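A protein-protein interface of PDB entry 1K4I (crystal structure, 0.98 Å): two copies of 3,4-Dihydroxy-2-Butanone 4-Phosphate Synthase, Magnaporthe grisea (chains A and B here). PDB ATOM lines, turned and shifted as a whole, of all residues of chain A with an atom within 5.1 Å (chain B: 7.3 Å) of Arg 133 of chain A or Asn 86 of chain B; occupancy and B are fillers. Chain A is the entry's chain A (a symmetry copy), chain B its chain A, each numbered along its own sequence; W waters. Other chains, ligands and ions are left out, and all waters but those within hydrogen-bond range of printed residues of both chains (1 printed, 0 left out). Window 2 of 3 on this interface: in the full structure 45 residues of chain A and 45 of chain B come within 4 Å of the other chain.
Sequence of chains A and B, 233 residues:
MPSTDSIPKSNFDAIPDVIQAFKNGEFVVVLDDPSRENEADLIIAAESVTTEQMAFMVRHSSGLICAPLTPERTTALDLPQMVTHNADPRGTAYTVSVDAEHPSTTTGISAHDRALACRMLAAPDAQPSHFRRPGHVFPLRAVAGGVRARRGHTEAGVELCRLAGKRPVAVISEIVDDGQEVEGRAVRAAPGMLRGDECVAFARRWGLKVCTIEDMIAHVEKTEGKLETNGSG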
ATOM      1  N   LEU A  77       9.064 -33.697 -28.536  1.00  0.00           N
ATOM      2  CA  LEU A  77       9.762 -32.795 -27.634  1.00  0.00           C
ATOM      3  C   LEU A  77       8.874 -32.009 -26.725  1.00  0.00           C
ATOM      4  O   LEU A  77       9.348 -31.182 -25.942  1.00  0.00           O
ATOM      5  CB  LEU A  77      10.734 -31.862 -28.393  1.00  0.00           C
ATOM      6  CG  LEU A  77      11.690 -32.634 -29.316  1.00  0.00           C
ATOM      7  CD1 LEU A  77      12.652 -31.663 -29.995  1.00  0.00           C
ATOM      8  CD2 LEU A  77      12.450 -33.674 -28.527  1.00  0.00           C
ATOM      9  N   ASP A  78       7.565 -32.254 -26.839  1.00  0.00           N
ATOM     10  CA  ASP A  78       6.574 -31.595 -25.979  1.00  0.00           C
ATOM     11  C   ASP A  78       6.624 -30.090 -26.088  1.00  0.00           C
ATOM     12  O   ASP A  78       6.815 -29.357 -25.104  1.00  0.00           O
ATOM     13  CB  ASP A  78       6.715 -32.064 -24.510  1.00  0.00           C
ATOM     14  CG  ASP A  78       5.448 -31.809 -23.734  1.00  0.00           C
ATOM     15  OD1 ASP A  78       4.427 -31.354 -24.217  1.00  0.00           O
ATOM     16  OD2 ASP A  78       5.590 -32.039 -22.444  1.00  0.00           O
ATOM     17  N   LEU A  79       6.408 -29.621 -27.314  1.00  0.00           N
ATOM     18  CA  LEU A  79       6.414 -28.198 -27.628  1.00  0.00           C
ATOM     19  C   LEU A  79       5.055 -27.759 -28.165  1.00  0.00           C
ATOM     20  O   LEU A  79       4.794 -27.741 -29.370  1.00  0.00           O
ATOM     21  CB  LEU A  79       7.506 -27.898 -28.687  1.00  0.00           C
ATOM     22  CG  LEU A  79       8.909 -28.309 -28.257  1.00  0.00           C
ATOM     23  CD1 LEU A  79       9.839 -28.284 -29.468  1.00  0.00           C
ATOM     24  CD2 LEU A  79       9.410 -27.385 -27.168  1.00  0.00           C
ATOM     25  N   PRO A  80       4.148 -27.379 -27.264  1.00  0.00           N
ATOM     26  CA  PRO A  80       2.821 -26.979 -27.716  1.00  0.00           C
ATOM     27  C   PRO A  80       2.843 -25.597 -28.358  1.00  0.00           C
ATOM     28  O   PRO A  80       3.756 -24.796 -28.131  1.00  0.00           O
ATOM     29  CB  PRO A  80       1.962 -26.915 -26.432  1.00  0.00           C
ATOM     30  CG  PRO A  80       2.965 -26.851 -25.279  1.00  0.00           C
ATOM     31  CD  PRO A  80       4.292 -27.451 -25.786  1.00  0.00           C
ATOM     32  N   VAL A  96       5.880 -22.845 -27.810  1.00  0.00           N
ATOM     33  CA  VAL A  96       6.456 -22.159 -26.678  1.00  0.00           C
ATOM     34  C   VAL A  96       7.995 -22.072 -26.973  1.00  0.00           C
ATOM     35  O   VAL A  96       8.558 -22.939 -27.649  1.00  0.00           O
ATOM     36  CB  VAL A  96       6.188 -22.977 -25.398  1.00  0.00           C
ATOM     37  CG1 VAL A  96       6.798 -24.360 -25.510  1.00  0.00           C
ATOM     38  CG2 VAL A  96       6.801 -22.276 -24.215  1.00  0.00           C
ATOM     39  N   SER A  97       8.638 -21.002 -26.507  1.00  0.00           N
ATOM     40  CA  SER A  97      10.065 -20.786 -26.742  1.00  0.00           C
ATOM     41  C   SER A  97      10.902 -21.631 -25.784  1.00  0.00           C
ATOM     42  O   SER A  97      10.427 -22.120 -24.744  1.00  0.00           O
ATOM     43  CB  SER A  97      10.376 -19.323 -26.585  1.00  0.00           C
ATOM     44  OG  SER A  97       9.937 -18.938 -25.283  1.00  0.00           O
ATOM     45  N   VAL A  98      12.179 -21.799 -26.155  1.00  0.00           N
ATOM     46  CA  VAL A  98      13.064 -22.658 -25.397  1.00  0.00           C
ATOM     47  C   VAL A  98      14.474 -22.105 -25.271  1.00  0.00           C
ATOM     48  O   VAL A  98      14.972 -21.343 -26.093  1.00  0.00           O
ATOM     49  CB  VAL A  98      13.204 -24.059 -26.073  1.00  0.00           C
ATOM     50  CG1 VAL A  98      11.861 -24.791 -26.149  1.00  0.00           C
ATOM     51  CG2 VAL A  98      13.868 -23.999 -27.479  1.00  0.00           C
ATOM     52  N   PRO A 128      11.995 -33.948 -24.116  1.00  0.00           N
ATOM     53  CA  PRO A 128      11.405 -32.709 -23.577  1.00  0.00           C
ATOM     54  C   PRO A 128      12.232 -32.045 -22.501  1.00  0.00           C
ATOM     55  O   PRO A 128      12.338 -30.810 -22.473  1.00  0.00           O
ATOM     56  CB  PRO A 128      10.026 -33.132 -23.052  1.00  0.00           C
ATOM     57  CG  PRO A 128       9.672 -34.317 -23.929  1.00  0.00           C
ATOM     58  CD  PRO A 128      10.986 -35.052 -24.154  1.00  0.00           C
ATOM     59  N   SER A 129      12.814 -32.829 -21.590  1.00  0.00           N
ATOM     60  CA  SER A 129      13.568 -32.289 -20.482  1.00  0.00           C
ATOM     61  C   SER A 129      14.864 -31.589 -20.891  1.00  0.00           C
ATOM     62  O   SER A 129      15.529 -30.936 -20.054  1.00  0.00           O
ATOM     63  CB  SER A 129      13.836 -33.389 -19.444  1.00  0.00           C
ATOM     64  OG  SER A 129      14.714 -34.351 -20.008  1.00  0.00           O
ATOM     65  N   PHE A 131      14.978 -29.054 -22.742  1.00  0.00           N
ATOM     66  CA  PHE A 131      14.676 -27.661 -23.013  1.00  0.00           C
ATOM     67  C   PHE A 131      13.969 -27.004 -21.861  1.00  0.00           C
ATOM     68  O   PHE A 131      13.042 -27.567 -21.286  1.00  0.00           O
ATOM     69  CB  PHE A 131      13.733 -27.589 -24.231  1.00  0.00           C
ATOM     70  CG  PHE A 131      14.389 -28.352 -25.356  1.00  0.00           C
ATOM     71  CD1 PHE A 131      13.989 -29.659 -25.651  1.00  0.00           C
ATOM     72  CD2 PHE A 131      15.464 -27.803 -26.065  1.00  0.00           C
ATOM     73  CE1 PHE A 131      14.663 -30.428 -26.602  1.00  0.00           C
ATOM     74  CE2 PHE A 131      16.126 -28.551 -27.042  1.00  0.00           C
ATOM     75  CZ  PHE A 131      15.758 -29.878 -27.280  1.00  0.00           C
ATOM     76  N   ARG A 132      14.400 -25.783 -21.566  1.00  0.00           N
ATOM     77  CA  ARG A 132      13.754 -24.970 -20.560  1.00  0.00           C
ATOM     78  C   ARG A 132      12.724 -24.130 -21.314  1.00  0.00           C
ATOM     79  O   ARG A 132      13.041 -23.619 -22.414  1.00  0.00           O
ATOM     80  CB  ARG A 132      14.773 -23.986 -19.982  1.00  0.00           C
ATOM     81  CG  ARG A 132      15.897 -24.672 -19.220  1.00  0.00           C
ATOM     82  CD  ARG A 132      16.953 -23.667 -18.737  1.00  0.00           C
ATOM     83  NE  ARG A 132      18.093 -24.367 -18.182  1.00  0.00           N
ATOM     84  CZ  ARG A 132      19.294 -23.813 -17.982  1.00  0.00           C
ATOM     85  NH1 ARG A 132      19.523 -22.534 -18.293  1.00  0.00           N
ATOM     86  NH2 ARG A 132      20.292 -24.550 -17.463  1.00  0.00           N
ATOM     87  N   ARG A 133      11.527 -23.949 -20.781  1.00  0.00           N
ATOM     88  CA  ARG A 133      10.511 -23.104 -21.408  1.00  0.00           C
ATOM     89  C   ARG A 133      10.067 -22.060 -20.366  1.00  0.00           C
ATOM     90  O   ARG A 133       9.872 -22.415 -19.184  1.00  0.00           O
ATOM     91  CB  ARG A 133       9.293 -23.924 -21.778  1.00  0.00           C
ATOM     92  CG  ARG A 133       9.664 -25.208 -22.570  1.00  0.00           C
ATOM     93  CD  ARG A 133       9.899 -26.416 -21.597  1.00  0.00           C
ATOM     94  NE  ARG A 133      10.351 -27.704 -22.186  1.00  0.00           N
ATOM     95  CZ  ARG A 133       9.602 -28.301 -23.101  1.00  0.00           C
ATOM     96  NH1 ARG A 133       8.410 -27.801 -23.456  1.00  0.00           N
ATOM     97  NH2 ARG A 133      10.049 -29.413 -23.672  1.00  0.00           N
ATOM     98  N   PRO A 134       9.895 -20.791 -20.718  1.00  0.00           N
ATOM     99  CA  PRO A 134      10.125 -20.208 -22.024  1.00  0.00           C
ATOM    100  C   PRO A 134      11.626 -19.945 -22.162  1.00  0.00           C
ATOM    101  O   PRO A 134      12.430 -20.214 -21.266  1.00  0.00           O
ATOM    102  CB  PRO A 134       9.375 -18.879 -21.947  1.00  0.00           C
ATOM    103  CG  PRO A 134       9.432 -18.497 -20.474  1.00  0.00           C
ATOM    104  CD  PRO A 134       9.441 -19.805 -19.694  1.00  0.00           C
ATOM    105  N   GLY A 135      12.013 -19.444 -23.322  1.00  0.00           N
ATOM    106  CA  GLY A 135      13.404 -19.193 -23.588  1.00  0.00           C
ATOM    107  C   GLY A 135      13.575 -18.209 -24.751  1.00  0.00           C
ATOM    108  O   GLY A 135      12.694 -17.382 -25.035  1.00  0.00           O
ATOM    109  N   GLN B  81       0.640 -14.651 -19.542  1.00  0.00           N
ATOM    110  CA  GLN B  81       1.971 -15.226 -19.593  1.00  0.00           C
ATOM    111  C   GLN B  81       2.051 -16.324 -20.656  1.00  0.00           C
ATOM    112  O   GLN B  81       1.116 -17.116 -20.858  1.00  0.00           O
ATOM    113  CB  GLN B  81       2.382 -15.811 -18.236  1.00  0.00           C
ATOM    114  CG  GLN B  81       2.631 -14.700 -17.205  1.00  0.00           C
ATOM    115  CD  GLN B  81       3.823 -13.869 -17.627  1.00  0.00           C
ATOM    116  OE1 GLN B  81       3.648 -12.683 -18.009  1.00  0.00           O
ATOM    117  NE2 GLN B  81       5.005 -14.431 -17.516  1.00  0.00           N
ATOM    118  N   MET B  82       3.175 -16.366 -21.365  1.00  0.00           N
ATOM    119  CA  MET B  82       3.357 -17.362 -22.396  1.00  0.00           C
ATOM    120  C   MET B  82       3.278 -18.766 -21.785  1.00  0.00           C
ATOM    121  O   MET B  82       2.737 -19.716 -22.386  1.00  0.00           O
ATOM    122  CB  MET B  82       4.739 -17.146 -23.038  1.00  0.00           C
ATOM    123  CG  MET B  82       4.929 -17.948 -24.310  1.00  0.00           C
ATOM    124  SD  MET B  82       6.669 -17.868 -24.842  1.00  0.00           S
ATOM    125  CE  MET B  82       6.700 -16.182 -25.479  1.00  0.00           C
ATOM    126  N   VAL B  83       3.885 -18.954 -20.632  1.00  0.00           N
ATOM    127  CA  VAL B  83       3.805 -20.269 -20.015  1.00  0.00           C
ATOM    128  C   VAL B  83       3.269 -20.165 -18.602  1.00  0.00           C
ATOM    129  O   VAL B  83       3.657 -19.279 -17.829  1.00  0.00           O
ATOM    130  CB  VAL B  83       5.034 -21.163 -20.106  1.00  0.00           C
ATOM    131  CG1 VAL B  83       6.014 -20.818 -21.227  1.00  0.00           C
ATOM    132  CG2 VAL B  83       5.692 -21.368 -18.763  1.00  0.00           C
ATOM    133  N   THR B  84       2.377 -21.092 -18.266  1.00  0.00           N
ATOM    134  CA  THR B  84       1.814 -21.152 -16.926  1.00  0.00           C
ATOM    135  C   THR B  84       2.805 -21.697 -15.899  1.00  0.00           C
ATOM    136  O   THR B  84       2.856 -21.273 -14.756  1.00  0.00           O
ATOM    137  CB  THR B  84       0.619 -22.088 -16.984  1.00  0.00           C
ATOM    138  OG1 THR B  84       1.113 -23.378 -17.320  1.00  0.00           O
ATOM    139  CG2 THR B  84      -0.316 -21.505 -18.039  1.00  0.00           C
ATOM    140  N   HIS B  85       3.691 -22.635 -16.292  1.00  0.00           N
ATOM    141  CA  HIS B  85       4.692 -23.149 -15.346  1.00  0.00           C
ATOM    142  C   HIS B  85       6.116 -22.682 -15.757  1.00  0.00           C
ATOM    143  O   HIS B  85       6.807 -23.481 -16.441  1.00  0.00           O
ATOM    144  CB  HIS B  85       4.659 -24.692 -15.258  1.00  0.00           C
ATOM    145  CG  HIS B  85       3.306 -25.288 -14.972  1.00  0.00           C
ATOM    146  ND1 HIS B  85       2.679 -25.139 -13.741  1.00  0.00           N
ATOM    147  CD2 HIS B  85       2.486 -26.049 -15.762  1.00  0.00           C
ATOM    148  CE1 HIS B  85       1.520 -25.794 -13.804  1.00  0.00           C
ATOM    149  NE2 HIS B  85       1.371 -26.358 -15.011  1.00  0.00           N
ATOM    150  N   ASN B  86       6.463 -21.420 -15.532  1.00  0.00           N
ATOM    151  CA  ASN B  86       7.752 -20.837 -15.961  1.00  0.00           C
ATOM    152  C   ASN B  86       9.057 -21.522 -15.607  1.00  0.00           C
ATOM    153  O   ASN B  86       9.447 -21.503 -14.443  1.00  0.00           O
ATOM    154  CB  ASN B  86       7.759 -19.346 -15.676  1.00  0.00           C
ATOM    155  CG  ASN B  86       8.848 -18.595 -16.396  1.00  0.00           C
ATOM    156  OD1 ASN B  86      10.018 -19.015 -16.324  1.00  0.00           O
ATOM    157  ND2 ASN B  86       8.465 -17.486 -17.079  1.00  0.00           N
ATOM    158  N   ALA B  87       9.749 -22.109 -16.608  1.00  0.00           N
ATOM    159  CA  ALA B  87      11.007 -22.831 -16.367  1.00  0.00           C
ATOM    160  C   ALA B  87      12.244 -21.988 -16.528  1.00  0.00           C
ATOM    161  O   ALA B  87      13.355 -22.502 -16.442  1.00  0.00           O
ATOM    162  CB  ALA B  87      11.145 -24.176 -17.103  1.00  0.00           C
ATOM    163  N   ASP B  88      12.056 -20.699 -16.785  1.00  0.00           N
ATOM    164  CA  ASP B  88      13.174 -19.761 -16.888  1.00  0.00           C
ATOM    165  C   ASP B  88      13.791 -19.575 -15.495  1.00  0.00           C
ATOM    166  O   ASP B  88      13.102 -19.391 -14.482  1.00  0.00           O
ATOM    167  CB  ASP B  88      12.714 -18.402 -17.435  1.00  0.00           C
ATOM    168  CG  ASP B  88      13.831 -17.383 -17.587  1.00  0.00           C
ATOM    169  OD1 ASP B  88      14.238 -16.684 -16.672  1.00  0.00           O
ATOM    170  OD2 ASP B  88      14.289 -17.291 -18.817  1.00  0.00           O
ATOM    171  N   PRO B  89      15.104 -19.655 -15.392  1.00  0.00           N
ATOM    172  CA  PRO B  89      15.733 -19.552 -14.081  1.00  0.00           C
ATOM    173  C   PRO B  89      15.598 -18.220 -13.377  1.00  0.00           C
ATOM    174  O   PRO B  89      15.731 -18.150 -12.160  1.00  0.00           O
ATOM    175  CB  PRO B  89      17.179 -20.036 -14.197  1.00  0.00           C
ATOM    176  CG  PRO B  89      17.344 -20.511 -15.635  1.00  0.00           C
ATOM    177  CD  PRO B  89      16.058 -20.212 -16.402  1.00  0.00           C
ATOM    178  N   ARG B  90      15.326 -17.176 -14.151  1.00  0.00           N
ATOM    179  CA  ARG B  90      15.120 -15.856 -13.576  1.00  0.00           C
ATOM    180  C   ARG B  90      13.628 -15.518 -13.512  1.00  0.00           C
ATOM    181  O   ARG B  90      13.133 -14.568 -12.909  1.00  0.00           O
ATOM    182  CB  ARG B  90      15.965 -14.821 -14.300  1.00  0.00           C
ATOM    183  CG  ARG B  90      17.418 -15.256 -14.228  1.00  0.00           C
ATOM    184  CD  ARG B  90      18.406 -14.103 -14.275  1.00  0.00           C
ATOM    185  NE  ARG B  90      19.543 -14.298 -13.376  1.00  0.00           N
ATOM    186  CZ  ARG B  90      20.641 -14.952 -13.700  1.00  0.00           C
ATOM    187  NH1 ARG B  90      20.821 -15.503 -14.918  1.00  0.00           N
ATOM    188  NH2 ARG B  90      21.615 -15.065 -12.785  1.00  0.00           N
ATOM    189  N   GLY B  91      12.868 -16.367 -14.139  1.00  0.00           N
ATOM    190  CA  GLY B  91      11.497 -16.102 -14.132  1.00  0.00           C
ATOM    191  C   GLY B  91      11.213 -14.983 -15.125  1.00  0.00           C
ATOM    192  O   GLY B  91      10.235 -14.336 -14.878  1.00  0.00           O
ATOM    193  N   THR B  92      11.975 -14.763 -16.207  1.00  0.00           N
ATOM    194  CA  THR B  92      11.601 -13.690 -17.164  1.00  0.00           C
ATOM    195  C   THR B  92      10.153 -13.912 -17.566  1.00  0.00           C
ATOM    196  O   THR B  92       9.767 -14.987 -18.029  1.00  0.00           O
ATOM    197  CB  THR B  92      12.464 -13.695 -18.422  1.00  0.00           C
ATOM    198  OG1 THR B  92      13.824 -13.621 -18.034  1.00  0.00           O
ATOM    199  CG2 THR B  92      12.056 -12.518 -19.300  1.00  0.00           C
ATOM    200  N   ALA B  93       9.326 -12.904 -17.312  1.00  0.00           N
ATOM    201  CA  ALA B  93       7.898 -13.032 -17.454  1.00  0.00           C
ATOM    202  C   ALA B  93       7.305 -12.707 -18.810  1.00  0.00           C
ATOM    203  O   ALA B  93       6.535 -11.753 -18.973  1.00  0.00           O
ATOM    204  CB  ALA B  93       7.292 -12.215 -16.328  1.00  0.00           C
ATOM    205  N   TYR B  94       7.699 -13.505 -19.808  1.00  0.00           N
ATOM    206  CA  TYR B  94       7.203 -13.271 -21.134  1.00  0.00           C
ATOM    207  C   TYR B  94       5.698 -13.430 -21.235  1.00  0.00           C
ATOM    208  O   TYR B  94       5.176 -14.448 -20.762  1.00  0.00           O
ATOM    209  CB  TYR B  94       7.733 -14.345 -22.122  1.00  0.00           C
ATOM    210  CG  TYR B  94       9.234 -14.290 -22.278  1.00  0.00           C
ATOM    211  CD1 TYR B  94      10.028 -15.194 -21.566  1.00  0.00           C
ATOM    212  CD2 TYR B  94       9.815 -13.377 -23.152  1.00  0.00           C
ATOM    213  CE1 TYR B  94      11.415 -15.134 -21.677  1.00  0.00           C
ATOM    214  CE2 TYR B  94      11.197 -13.336 -23.300  1.00  0.00           C
ATOM    215  CZ  TYR B  94      11.980 -14.222 -22.558  1.00  0.00           C
ATOM    216  OH  TYR B  94      13.360 -14.168 -22.716  1.00  0.00           O
HETATM  217  O   HOH W   1      14.920 -20.169 -20.046  1.00  0.00           O
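N of Met 82 of chain B lies within hydrogen-bond range of O of Tyr 94 of chain B. The backbone carbonyl oxygen of Thr 92 of chain B sits at hydrogen-bond distance from the side-chain amide nitrogen of Asn 86 of chain B, 3.0 Å away. N of Thr 92 of chain B lies within hydrogen-bond range of OD1 of Asp 88 of chain B, at 3.0 Å. O of Leu 77 of chain A lies within hydrogen-bond range of NH2 of Arg 133 of chain A (3.0 Å). The side-chain hydroxyl of Ser 97 of chain A is in hydrogen-bond range of the backbone NH of Gly 135 of chain A. NH2 of Arg 133 of chain A is in hydrogen-bond range of O of Pro 128 of chain A (2.9 Å).
No position is printed for both chains.
The side-chain sulfur of Met 82 of chain B lies within hydrogen-bond range of the side-chain hydroxyl of Ser 97 of chain A, 3.5 Å away. The backbone NH of Ala 87 of chain B is in hydrogen-bond range of the backbone carbonyl oxygen of Arg 133 of chain A (2.6 Å).
Hydrophobic or aromatic side chains of chain A within 4 Å of the printed part of chain B: Val 96 and Pro 134. Hydrophobic or aromatic side chains of chain B that line the printed part of chain A: Met 82, Val 83, Ala 87, Pro 89 and Tyr 94. Among the printed residues, no Asp or Glu carboxylate lies within 4 Å of a Lys or Arg side-chain nitrogen of the other chain.
Water W1 lies within hydrogen-bond range of the backbone carbonyl oxygen (O) of Pro 134 of chain A and the side-chain carboxylate (OD2) of Asp 88 of chain B.
Asn 86 of chain B touches just these residues of chain A: Arg 133 (3.8 Å) and Pro 134 (3.5 Å). Of the printed residues of chain A, Pro 89 of chain B touches Arg 132 (3.99 Å). Printed residues of chain A within 4 Å of Val 83 of chain B: Val 96 (3.4 Å) and Pro 134 (3.9 Å). Of the printed residues of chain B, Arg 132 of chain A touches Pro 89 (3.99 Å). Of the printed residues of chain A, Met 82 of chain B touches Ser 97 (3.5 Å). The nearest printed residue of chain A that does not touch Met 82 of chain B is Pro 134 of chain A (4.1 Å).
Val 96 of chain A touches Val 83 of chain B (CG2 to CG1, 3.4 Å). Pro 89 of chain B touches Arg 132 of chain A (CG to NH1, 3.99 Å). O of Arg 133 of chain A touches C of Asn 86 of chain B, 3.8 Å away. Arg 133 of chain A touches Asp 88 of chain B (O to N, 3.7 Å). CD of Pro 134 of chain A touches CG1 of Val 83 of chain B (3.9 Å). CD of Pro 134 of chain A touches OD1 of Asn 86 of chain B (3.5 Å). CD of Pro 134 of chain A touches N of Ala 87 of chain B, 3.9 Å away. Pro 134 of chain A touches Tyr 94 of chain B.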
